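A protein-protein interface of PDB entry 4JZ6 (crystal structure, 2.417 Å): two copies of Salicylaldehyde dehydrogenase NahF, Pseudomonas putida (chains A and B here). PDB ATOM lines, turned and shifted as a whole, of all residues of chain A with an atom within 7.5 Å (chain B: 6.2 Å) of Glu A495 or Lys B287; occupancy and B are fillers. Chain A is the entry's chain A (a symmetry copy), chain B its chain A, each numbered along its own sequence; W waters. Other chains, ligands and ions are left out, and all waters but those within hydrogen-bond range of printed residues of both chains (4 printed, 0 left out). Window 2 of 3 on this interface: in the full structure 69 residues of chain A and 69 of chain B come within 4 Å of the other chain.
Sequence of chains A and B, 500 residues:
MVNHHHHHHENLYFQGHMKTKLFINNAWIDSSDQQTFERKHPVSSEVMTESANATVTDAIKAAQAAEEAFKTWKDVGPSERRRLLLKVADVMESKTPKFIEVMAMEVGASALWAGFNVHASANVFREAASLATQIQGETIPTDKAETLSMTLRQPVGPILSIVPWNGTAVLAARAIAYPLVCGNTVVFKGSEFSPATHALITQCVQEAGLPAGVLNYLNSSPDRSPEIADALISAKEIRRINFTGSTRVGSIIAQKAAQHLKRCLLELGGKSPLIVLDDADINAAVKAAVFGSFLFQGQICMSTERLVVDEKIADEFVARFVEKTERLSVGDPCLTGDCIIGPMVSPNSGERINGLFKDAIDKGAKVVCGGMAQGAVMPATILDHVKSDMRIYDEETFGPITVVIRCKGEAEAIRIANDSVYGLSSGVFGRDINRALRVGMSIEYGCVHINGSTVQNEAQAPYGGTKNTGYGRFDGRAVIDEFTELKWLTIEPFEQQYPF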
ATOM      1  N   ALA A 145      -1.408   1.376  22.450  1.00  0.00           N
ATOM      2  CA  ALA A 145      -2.326   2.177  23.254  1.00  0.00           C
ATOM      3  C   ALA A 145      -3.595   1.403  23.598  1.00  0.00           C
ATOM      4  O   ALA A 145      -4.008   0.515  22.848  1.00  0.00           O
ATOM      5  CB  ALA A 145      -2.672   3.471  22.540  1.00  0.00           C
ATOM      6  N   GLU A 146      -4.199   1.754  24.734  1.00  0.00           N
ATOM      7  CA  GLU A 146      -5.468   1.179  25.176  1.00  0.00           C
ATOM      8  C   GLU A 146      -5.428  -0.344  25.196  1.00  0.00           C
ATOM      9  O   GLU A 146      -6.411  -1.004  24.855  1.00  0.00           O
ATOM     10  CB  GLU A 146      -6.616   1.666  24.291  1.00  0.00           C
ATOM     11  CG  GLU A 146      -6.778   3.168  24.287  1.00  0.00           C
ATOM     12  CD  GLU A 146      -7.936   3.629  23.433  1.00  0.00           C
ATOM     13  OE1 GLU A 146      -8.736   2.768  23.008  1.00  0.00           O
ATOM     14  OE2 GLU A 146      -8.052   4.851  23.185  1.00  0.00           O
ATOM     15  N   GLU A 492      -7.236  -5.676  23.569  1.00  0.00           N
ATOM     16  CA  GLU A 492      -6.931  -4.589  22.653  1.00  0.00           C
ATOM     17  C   GLU A 492      -8.180  -3.807  22.283  1.00  0.00           C
ATOM     18  O   GLU A 492      -9.293  -4.322  22.399  1.00  0.00           O
ATOM     19  CB  GLU A 492      -6.249  -5.157  21.406  1.00  0.00           C
ATOM     20  CG  GLU A 492      -5.040  -6.028  21.733  1.00  0.00           C
ATOM     21  CD  GLU A 492      -4.491  -6.756  20.521  1.00  0.00           C
ATOM     22  OE1 GLU A 492      -4.659  -6.238  19.395  1.00  0.00           O
ATOM     23  OE2 GLU A 492      -3.901  -7.848  20.692  1.00  0.00           O
ATOM     24  N   PRO A 493      -8.001  -2.542  21.857  1.00  0.00           N
ATOM     25  CA  PRO A 493      -9.143  -1.730  21.437  1.00  0.00           C
ATOM     26  C   PRO A 493      -9.758  -2.282  20.163  1.00  0.00           C
ATOM     27  O   PRO A 493      -9.090  -3.007  19.431  1.00  0.00           O
ATOM     28  CB  PRO A 493      -8.514  -0.355  21.174  1.00  0.00           C
ATOM     29  CG  PRO A 493      -7.085  -0.630  20.905  1.00  0.00           C
ATOM     30  CD  PRO A 493      -6.738  -1.786  21.778  1.00  0.00           C
ATOM     31  N   PHE A 494     -11.020  -1.960  19.907  1.00  0.00           N
ATOM     32  CA  PHE A 494     -11.657  -2.411  18.682  1.00  0.00           C
ATOM     33  C   PHE A 494     -10.978  -1.761  17.479  1.00  0.00           C
ATOM     34  O   PHE A 494     -10.595  -2.442  16.527  1.00  0.00           O
ATOM     35  CB  PHE A 494     -13.156  -2.106  18.700  1.00  0.00           C
ATOM     36  CG  PHE A 494     -13.880  -2.698  19.880  1.00  0.00           C
ATOM     37  CD1 PHE A 494     -13.873  -4.064  20.101  1.00  0.00           C
ATOM     38  CD2 PHE A 494     -14.571  -1.890  20.765  1.00  0.00           C
ATOM     39  CE1 PHE A 494     -14.533  -4.607  21.179  1.00  0.00           C
ATOM     40  CE2 PHE A 494     -15.236  -2.433  21.843  1.00  0.00           C
ATOM     41  CZ  PHE A 494     -15.217  -3.791  22.049  1.00  0.00           C
ATOM     42  N   GLU A 495     -10.800  -0.447  17.543  1.00  0.00           N
ATOM     43  CA  GLU A 495     -10.174   0.297  16.459  1.00  0.00           C
ATOM     44  C   GLU A 495      -8.654   0.339  16.592  1.00  0.00           C
ATOM     45  O   GLU A 495      -8.122   0.919  17.536  1.00  0.00           O
ATOM     46  CB  GLU A 495     -10.735   1.720  16.401  1.00  0.00           C
ATOM     47  CG  GLU A 495     -11.281   2.122  15.039  1.00  0.00           C
ATOM     48  CD  GLU A 495     -10.186   2.304  13.996  1.00  0.00           C
ATOM     49  OE1 GLU A 495      -9.254   3.103  14.237  1.00  0.00           O
ATOM     50  OE2 GLU A 495     -10.259   1.648  12.934  1.00  0.00           O
ATOM     51  N   GLN A 496      -7.963  -0.291  15.646  1.00  0.00           N
ATOM     52  CA  GLN A 496      -6.510  -0.161  15.532  1.00  0.00           C
ATOM     53  C   GLN A 496      -6.052  -0.205  14.063  1.00  0.00           C
ATOM     54  O   GLN A 496      -6.790  -0.653  13.186  1.00  0.00           O
ATOM     55  CB  GLN A 496      -5.780  -1.205  16.389  1.00  0.00           C
ATOM     56  CG  GLN A 496      -6.255  -2.633  16.207  1.00  0.00           C
ATOM     57  CD  GLN A 496      -5.620  -3.598  17.208  1.00  0.00           C
ATOM     58  OE1 GLN A 496      -4.437  -3.934  17.108  1.00  0.00           O
ATOM     59  NE2 GLN A 496      -6.409  -4.044  18.176  1.00  0.00           N
ATOM     60  N   GLN A 497      -4.839   0.278  13.804  1.00  0.00           N
ATOM     61  CA  GLN A 497      -4.331   0.410  12.439  1.00  0.00           C
ATOM     62  C   GLN A 497      -3.465  -0.766  11.994  1.00  0.00           C
ATOM     63  O   GLN A 497      -2.714  -1.339  12.786  1.00  0.00           O
ATOM     64  CB  GLN A 497      -3.533   1.706  12.296  1.00  0.00           C
ATOM     65  CG  GLN A 497      -4.336   2.968  12.549  1.00  0.00           C
ATOM     66  CD  GLN A 497      -5.359   3.242  11.462  1.00  0.00           C
ATOM     67  OE1 GLN A 497      -6.427   2.620  11.417  1.00  0.00           O
ATOM     68  NE2 GLN A 497      -5.040   4.182  10.577  1.00  0.00           N
ATOM     69  N   TYR A 498      -3.577  -1.112  10.715  1.00  0.00           N
ATOM     70  CA  TYR A 498      -2.752  -2.157  10.122  1.00  0.00           C
ATOM     71  C   TYR A 498      -2.089  -1.649   8.841  1.00  0.00           C
ATOM     72  O   TYR A 498      -2.674  -0.847   8.114  1.00  0.00           O
ATOM     73  CB  TYR A 498      -3.596  -3.399   9.826  1.00  0.00           C
ATOM     74  CG  TYR A 498      -4.184  -4.047  11.056  1.00  0.00           C
ATOM     75  CD1 TYR A 498      -3.494  -5.046  11.736  1.00  0.00           C
ATOM     76  CD2 TYR A 498      -5.433  -3.662  11.540  1.00  0.00           C
ATOM     77  CE1 TYR A 498      -4.029  -5.640  12.859  1.00  0.00           C
ATOM     78  CE2 TYR A 498      -5.972  -4.250  12.663  1.00  0.00           C
ATOM     79  CZ  TYR A 498      -5.266  -5.237  13.316  1.00  0.00           C
ATOM     80  OH  TYR A 498      -5.805  -5.828  14.435  1.00  0.00           O
ATOM     81  N   PHE A 500      -1.532  -2.996   5.936  1.00  0.00           N
ATOM     82  CA  PHE A 500      -2.287  -3.245   4.714  1.00  0.00           C
ATOM     83  C   PHE A 500      -3.667  -3.794   5.022  1.00  0.00           C
ATOM     84  O   PHE A 500      -4.069  -3.839   6.184  1.00  0.00           O
ATOM     85  CB  PHE A 500      -1.526  -4.191   3.784  1.00  0.00           C
ATOM     86  CG  PHE A 500      -1.182  -5.510   4.403  1.00  0.00           C
ATOM     87  CD1 PHE A 500       0.031  -5.695   5.037  1.00  0.00           C
ATOM     88  CD2 PHE A 500      -2.062  -6.573   4.332  1.00  0.00           C
ATOM     89  CE1 PHE A 500       0.354  -6.909   5.599  1.00  0.00           C
ATOM     90  CE2 PHE A 500      -1.741  -7.790   4.895  1.00  0.00           C
ATOM     91  CZ  PHE A 500      -0.531  -7.958   5.529  1.00  0.00           C
ATOM     92  OXT PHE A 500      -4.404  -4.187   4.118  1.00  0.00           O
ATOM     93  N   ASP B 281     -16.900  -7.293  16.193  1.00  0.00           N
ATOM     94  CA  ASP B 281     -16.770  -6.132  15.334  1.00  0.00           C
ATOM     95  C   ASP B 281     -16.202  -6.675  14.025  1.00  0.00           C
ATOM     96  O   ASP B 281     -14.998  -6.893  13.914  1.00  0.00           O
ATOM     97  CB  ASP B 281     -15.803  -5.136  15.982  1.00  0.00           C
ATOM     98  CG  ASP B 281     -15.606  -3.859  15.165  1.00  0.00           C
ATOM     99  OD1 ASP B 281     -15.894  -3.843  13.946  1.00  0.00           O
ATOM    100  OD2 ASP B 281     -15.134  -2.862  15.757  1.00  0.00           O
ATOM    101  N   ILE B 282     -17.070  -6.914  13.046  1.00  0.00           N
ATOM    102  CA  ILE B 282     -16.664  -7.568  11.803  1.00  0.00           C
ATOM    103  C   ILE B 282     -15.615  -6.766  11.032  1.00  0.00           C
ATOM    104  O   ILE B 282     -14.672  -7.335  10.473  1.00  0.00           O
ATOM    105  CB  ILE B 282     -17.878  -7.868  10.908  1.00  0.00           C
ATOM    106  CG1 ILE B 282     -18.867  -8.754  11.660  1.00  0.00           C
ATOM    107  CG2 ILE B 282     -17.454  -8.555   9.616  1.00  0.00           C
ATOM    108  CD1 ILE B 282     -20.101  -9.073  10.864  1.00  0.00           C
ATOM    109  N   ASN B 283     -15.774  -5.447  11.010  1.00  0.00           N
ATOM    110  CA  ASN B 283     -14.758  -4.580  10.429  1.00  0.00           C
ATOM    111  C   ASN B 283     -13.385  -4.867  11.037  1.00  0.00           C
ATOM    112  O   ASN B 283     -12.430  -5.177  10.324  1.00  0.00           O
ATOM    113  CB  ASN B 283     -15.126  -3.111  10.638  1.00  0.00           C
ATOM    114  CG  ASN B 283     -14.042  -2.165  10.155  1.00  0.00           C
ATOM    115  OD1 ASN B 283     -13.283  -1.606  10.953  1.00  0.00           O
ATOM    116  ND2 ASN B 283     -13.960  -1.986   8.841  1.00  0.00           N
ATOM    117  N   ALA B 284     -13.312  -4.788  12.361  1.00  0.00           N
ATOM    118  CA  ALA B 284     -12.065  -4.986  13.083  1.00  0.00           C
ATOM    119  C   ALA B 284     -11.496  -6.391  12.886  1.00  0.00           C
ATOM    120  O   ALA B 284     -10.277  -6.569  12.797  1.00  0.00           O
ATOM    121  CB  ALA B 284     -12.262  -4.695  14.559  1.00  0.00           C
ATOM    122  N   ALA B 285     -12.375  -7.385  12.827  1.00  0.00           N
ATOM    123  CA  ALA B 285     -11.937  -8.770  12.700  1.00  0.00           C
ATOM    124  C   ALA B 285     -11.388  -9.044  11.308  1.00  0.00           C
ATOM    125  O   ALA B 285     -10.377  -9.733  11.158  1.00  0.00           O
ATOM    126  CB  ALA B 285     -13.065  -9.728  13.030  1.00  0.00           C
ATOM    127  N   VAL B 286     -12.054  -8.502  10.291  1.00  0.00           N
ATOM    128  CA  VAL B 286     -11.576  -8.642   8.920  1.00  0.00           C
ATOM    129  C   VAL B 286     -10.169  -8.066   8.783  1.00  0.00           C
ATOM    130  O   VAL B 286      -9.288  -8.700   8.199  1.00  0.00           O
ATOM    131  CB  VAL B 286     -12.536  -7.992   7.898  1.00  0.00           C
ATOM    132  CG1 VAL B 286     -11.877  -7.886   6.531  1.00  0.00           C
ATOM    133  CG2 VAL B 286     -13.823  -8.798   7.800  1.00  0.00           C
ATOM    134  N   LYS B 287      -9.953  -6.883   9.351  1.00  0.00           N
ATOM    135  CA  LYS B 287      -8.636  -6.252   9.322  1.00  0.00           C
ATOM    136  C   LYS B 287      -7.566  -7.125   9.974  1.00  0.00           C
ATOM    137  O   LYS B 287      -6.475  -7.299   9.434  1.00  0.00           O
ATOM    138  CB  LYS B 287      -8.674  -4.864   9.971  1.00  0.00           C
ATOM    139  CG  LYS B 287      -9.564  -3.872   9.238  1.00  0.00           C
ATOM    140  CD  LYS B 287      -9.221  -2.428   9.563  1.00  0.00           C
ATOM    141  CE  LYS B 287      -9.732  -1.999  10.926  1.00  0.00           C
ATOM    142  NZ  LYS B 287      -9.391  -0.570  11.208  1.00  0.00           N
ATOM    143  N   ALA B 288      -7.883  -7.684  11.132  1.00  0.00           N
ATOM    144  CA  ALA B 288      -6.938  -8.563  11.805  1.00  0.00           C
ATOM    145  C   ALA B 288      -6.722  -9.815  10.973  1.00  0.00           C
ATOM    146  O   ALA B 288      -5.608 -10.329  10.881  1.00  0.00           O
ATOM    147  CB  ALA B 288      -7.437  -8.924  13.184  1.00  0.00           C
ATOM    148  N   ALA B 289      -7.800 -10.302  10.367  1.00  0.00           N
ATOM    149  CA  ALA B 289      -7.729 -11.508   9.557  1.00  0.00           C
ATOM    150  C   ALA B 289      -6.834 -11.289   8.338  1.00  0.00           C
ATOM    151  O   ALA B 289      -5.908 -12.063   8.097  1.00  0.00           O
ATOM    152  CB  ALA B 289      -9.123 -11.954   9.137  1.00  0.00           C
ATOM    153  N   VAL B 290      -7.111 -10.227   7.584  1.00  0.00           N
ATOM    154  CA  VAL B 290      -6.324  -9.892   6.398  1.00  0.00           C
ATOM    155  C   VAL B 290      -4.839  -9.766   6.727  1.00  0.00           C
ATOM    156  O   VAL B 290      -3.986 -10.301   6.014  1.00  0.00           O
ATOM    157  CB  VAL B 290      -6.821  -8.594   5.743  1.00  0.00           C
ATOM    158  CG1 VAL B 290      -5.868  -8.149   4.652  1.00  0.00           C
ATOM    159  CG2 VAL B 290      -8.204  -8.804   5.173  1.00  0.00           C
ATOM    160  N   PHE B 291      -4.541  -9.083   7.826  1.00  0.00           N
ATOM    161  CA  PHE B 291      -3.164  -8.861   8.240  1.00  0.00           C
ATOM    162  C   PHE B 291      -2.461 -10.148   8.661  1.00  0.00           C
ATOM    163  O   PHE B 291      -1.384 -10.472   8.151  1.00  0.00           O
ATOM    164  CB  PHE B 291      -3.117  -7.844   9.380  1.00  0.00           C
ATOM    165  CG  PHE B 291      -1.760  -7.694  10.004  1.00  0.00           C
ATOM    166  CD1 PHE B 291      -0.746  -7.027   9.339  1.00  0.00           C
ATOM    167  CD2 PHE B 291      -1.505  -8.204  11.263  1.00  0.00           C
ATOM    168  CE1 PHE B 291       0.501  -6.885   9.914  1.00  0.00           C
ATOM    169  CE2 PHE B 291      -0.264  -8.065  11.846  1.00  0.00           C
ATOM    170  CZ  PHE B 291       0.741  -7.406  11.171  1.00  0.00           C
ATOM    171  N   GLY B 292      -3.071 -10.869   9.599  1.00  0.00           N
ATOM    172  CA  GLY B 292      -2.470 -12.068  10.158  1.00  0.00           C
ATOM    173  C   GLY B 292      -2.351 -13.193   9.150  1.00  0.00           C
ATOM    174  O   GLY B 292      -1.452 -14.023   9.237  1.00  0.00           O
ATOM    175  N   SER B 453      -4.903  -9.442  16.227  1.00  0.00           N
ATOM    176  CA  SER B 453      -4.484 -10.430  15.237  1.00  0.00           C
ATOM    177  C   SER B 453      -3.725 -11.573  15.900  1.00  0.00           C
ATOM    178  O   SER B 453      -3.372 -11.492  17.078  1.00  0.00           O
ATOM    179  CB  SER B 453      -3.608  -9.781  14.162  1.00  0.00           C
ATOM    180  OG  SER B 453      -2.266  -9.646  14.600  1.00  0.00           O
HETATM  181  O   HOH W   1      -8.396  -5.040  14.390  1.00  0.00           O
HETATM  182  O   HOH W   2      -9.696  -1.975  14.209  1.00  0.00           O
HETATM  183  O   HOH W   3      -6.228  -5.131   7.421  1.00  0.00           O
HETATM  184  O   HOH W   4      -3.907  -6.700  16.840  1.00  0.00           O
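The side-chain amino group of Lys B287 is in salt-bridge range of the side-chain carboxylate of Glu A495 (2.9 Å).
The backbone carbonyl oxygen (O) of Gln A496 lies within hydrogen-bond range of the side-chain amino group (NZ) of Lys B287 (3.3 Å).
Among the printed residues, pairs that only touch across the chains: Phe A494 with Asp B281 (3.6 Å), Phe A494 with Ala B284 (3.4 Å), Tyr A498 with Lys B287 (3.8 Å), Tyr A498 with Ala B288 (3.7 Å), Tyr A498 with Phe B291 (3.6 Å), Phe A500 with Val B290 (3.5 Å) and Phe A500 with Phe B291 (3.7 Å).
Printed residues of chain B that touch a printed residue of chain A: Asp B281, Ala B284, Lys B287, Ala B288, Val B290 and Phe B291.
Hydrophobic or aromatic side chains of chain B within 4 Å of the printed part of chain A: Ala B284, Ala B288 and Phe B291.
Hydrophobic or aromatic side chains of chain A that line the printed part of chain B: Phe A494, Tyr A498 and Phe A500.
Among the printed residues, Asp or Glu carboxylates within 4 Å of a Lys or Arg side-chain nitrogen of the other chain: Glu A495 with Lys B287.
Of the printed residues of chain B, Phe A494 touches Asp B281 (3.6 Å) and Ala B284 (3.4 Å).
Of the printed residues of chain B, Glu A495 touches Lys B287.
Of the printed residues of chain B, Phe A500 touches Val B290 (3.5 Å) and Phe B291 (3.7 Å).
Printed residues of chain A within 4 Å of Asp B281: Phe A494.
Of chain A, only Glu A495, Gln A496 and Tyr A498 come within 4 Å of Lys B287.
The nearest residue of chain A that does not touch Lys B287 is Gln A497 (4.4 Å).
The nearest printed residue of chain A that does not touch Ala B284 is Tyr A498 (4.8 Å).
Water W2 lies within hydrogen-bond range of O of Phe A494, N of Gln A496 and NZ of Lys B287.
Water W4 lies within hydrogen-bond range of OE1 of Glu A492, OE1 of Gln A496, N of Ser B453 and OH of Tyr A498.
Water W1 lies within hydrogen-bond range of OH of Tyr A498 (2.7 Å) and O of Ala B284 (2.9 Å).
Water W3 bridges O of Phe A500 and O of Lys B287.
No position is printed for both chains.
Of the 9 pairs that touch across the chains among the printed residues, none has its exchanged pair printed and touching as well.
The side-chain carboxylate of Asp B281 sits close to the backbone NH of Asn B283.
OD1 of Asp B281 is in hydrogen-bond range of N of Ala B284.
The side-chain amide nitrogen (NE2) of Gln A496 sits at hydrogen-bond distance from the side-chain carboxylate (OE1) of Glu A492, at 3.1 Å.
The backbone carbonyl oxygen of Pro A493 is in hydrogen-bond range of the side-chain amide nitrogen of Gln A496.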
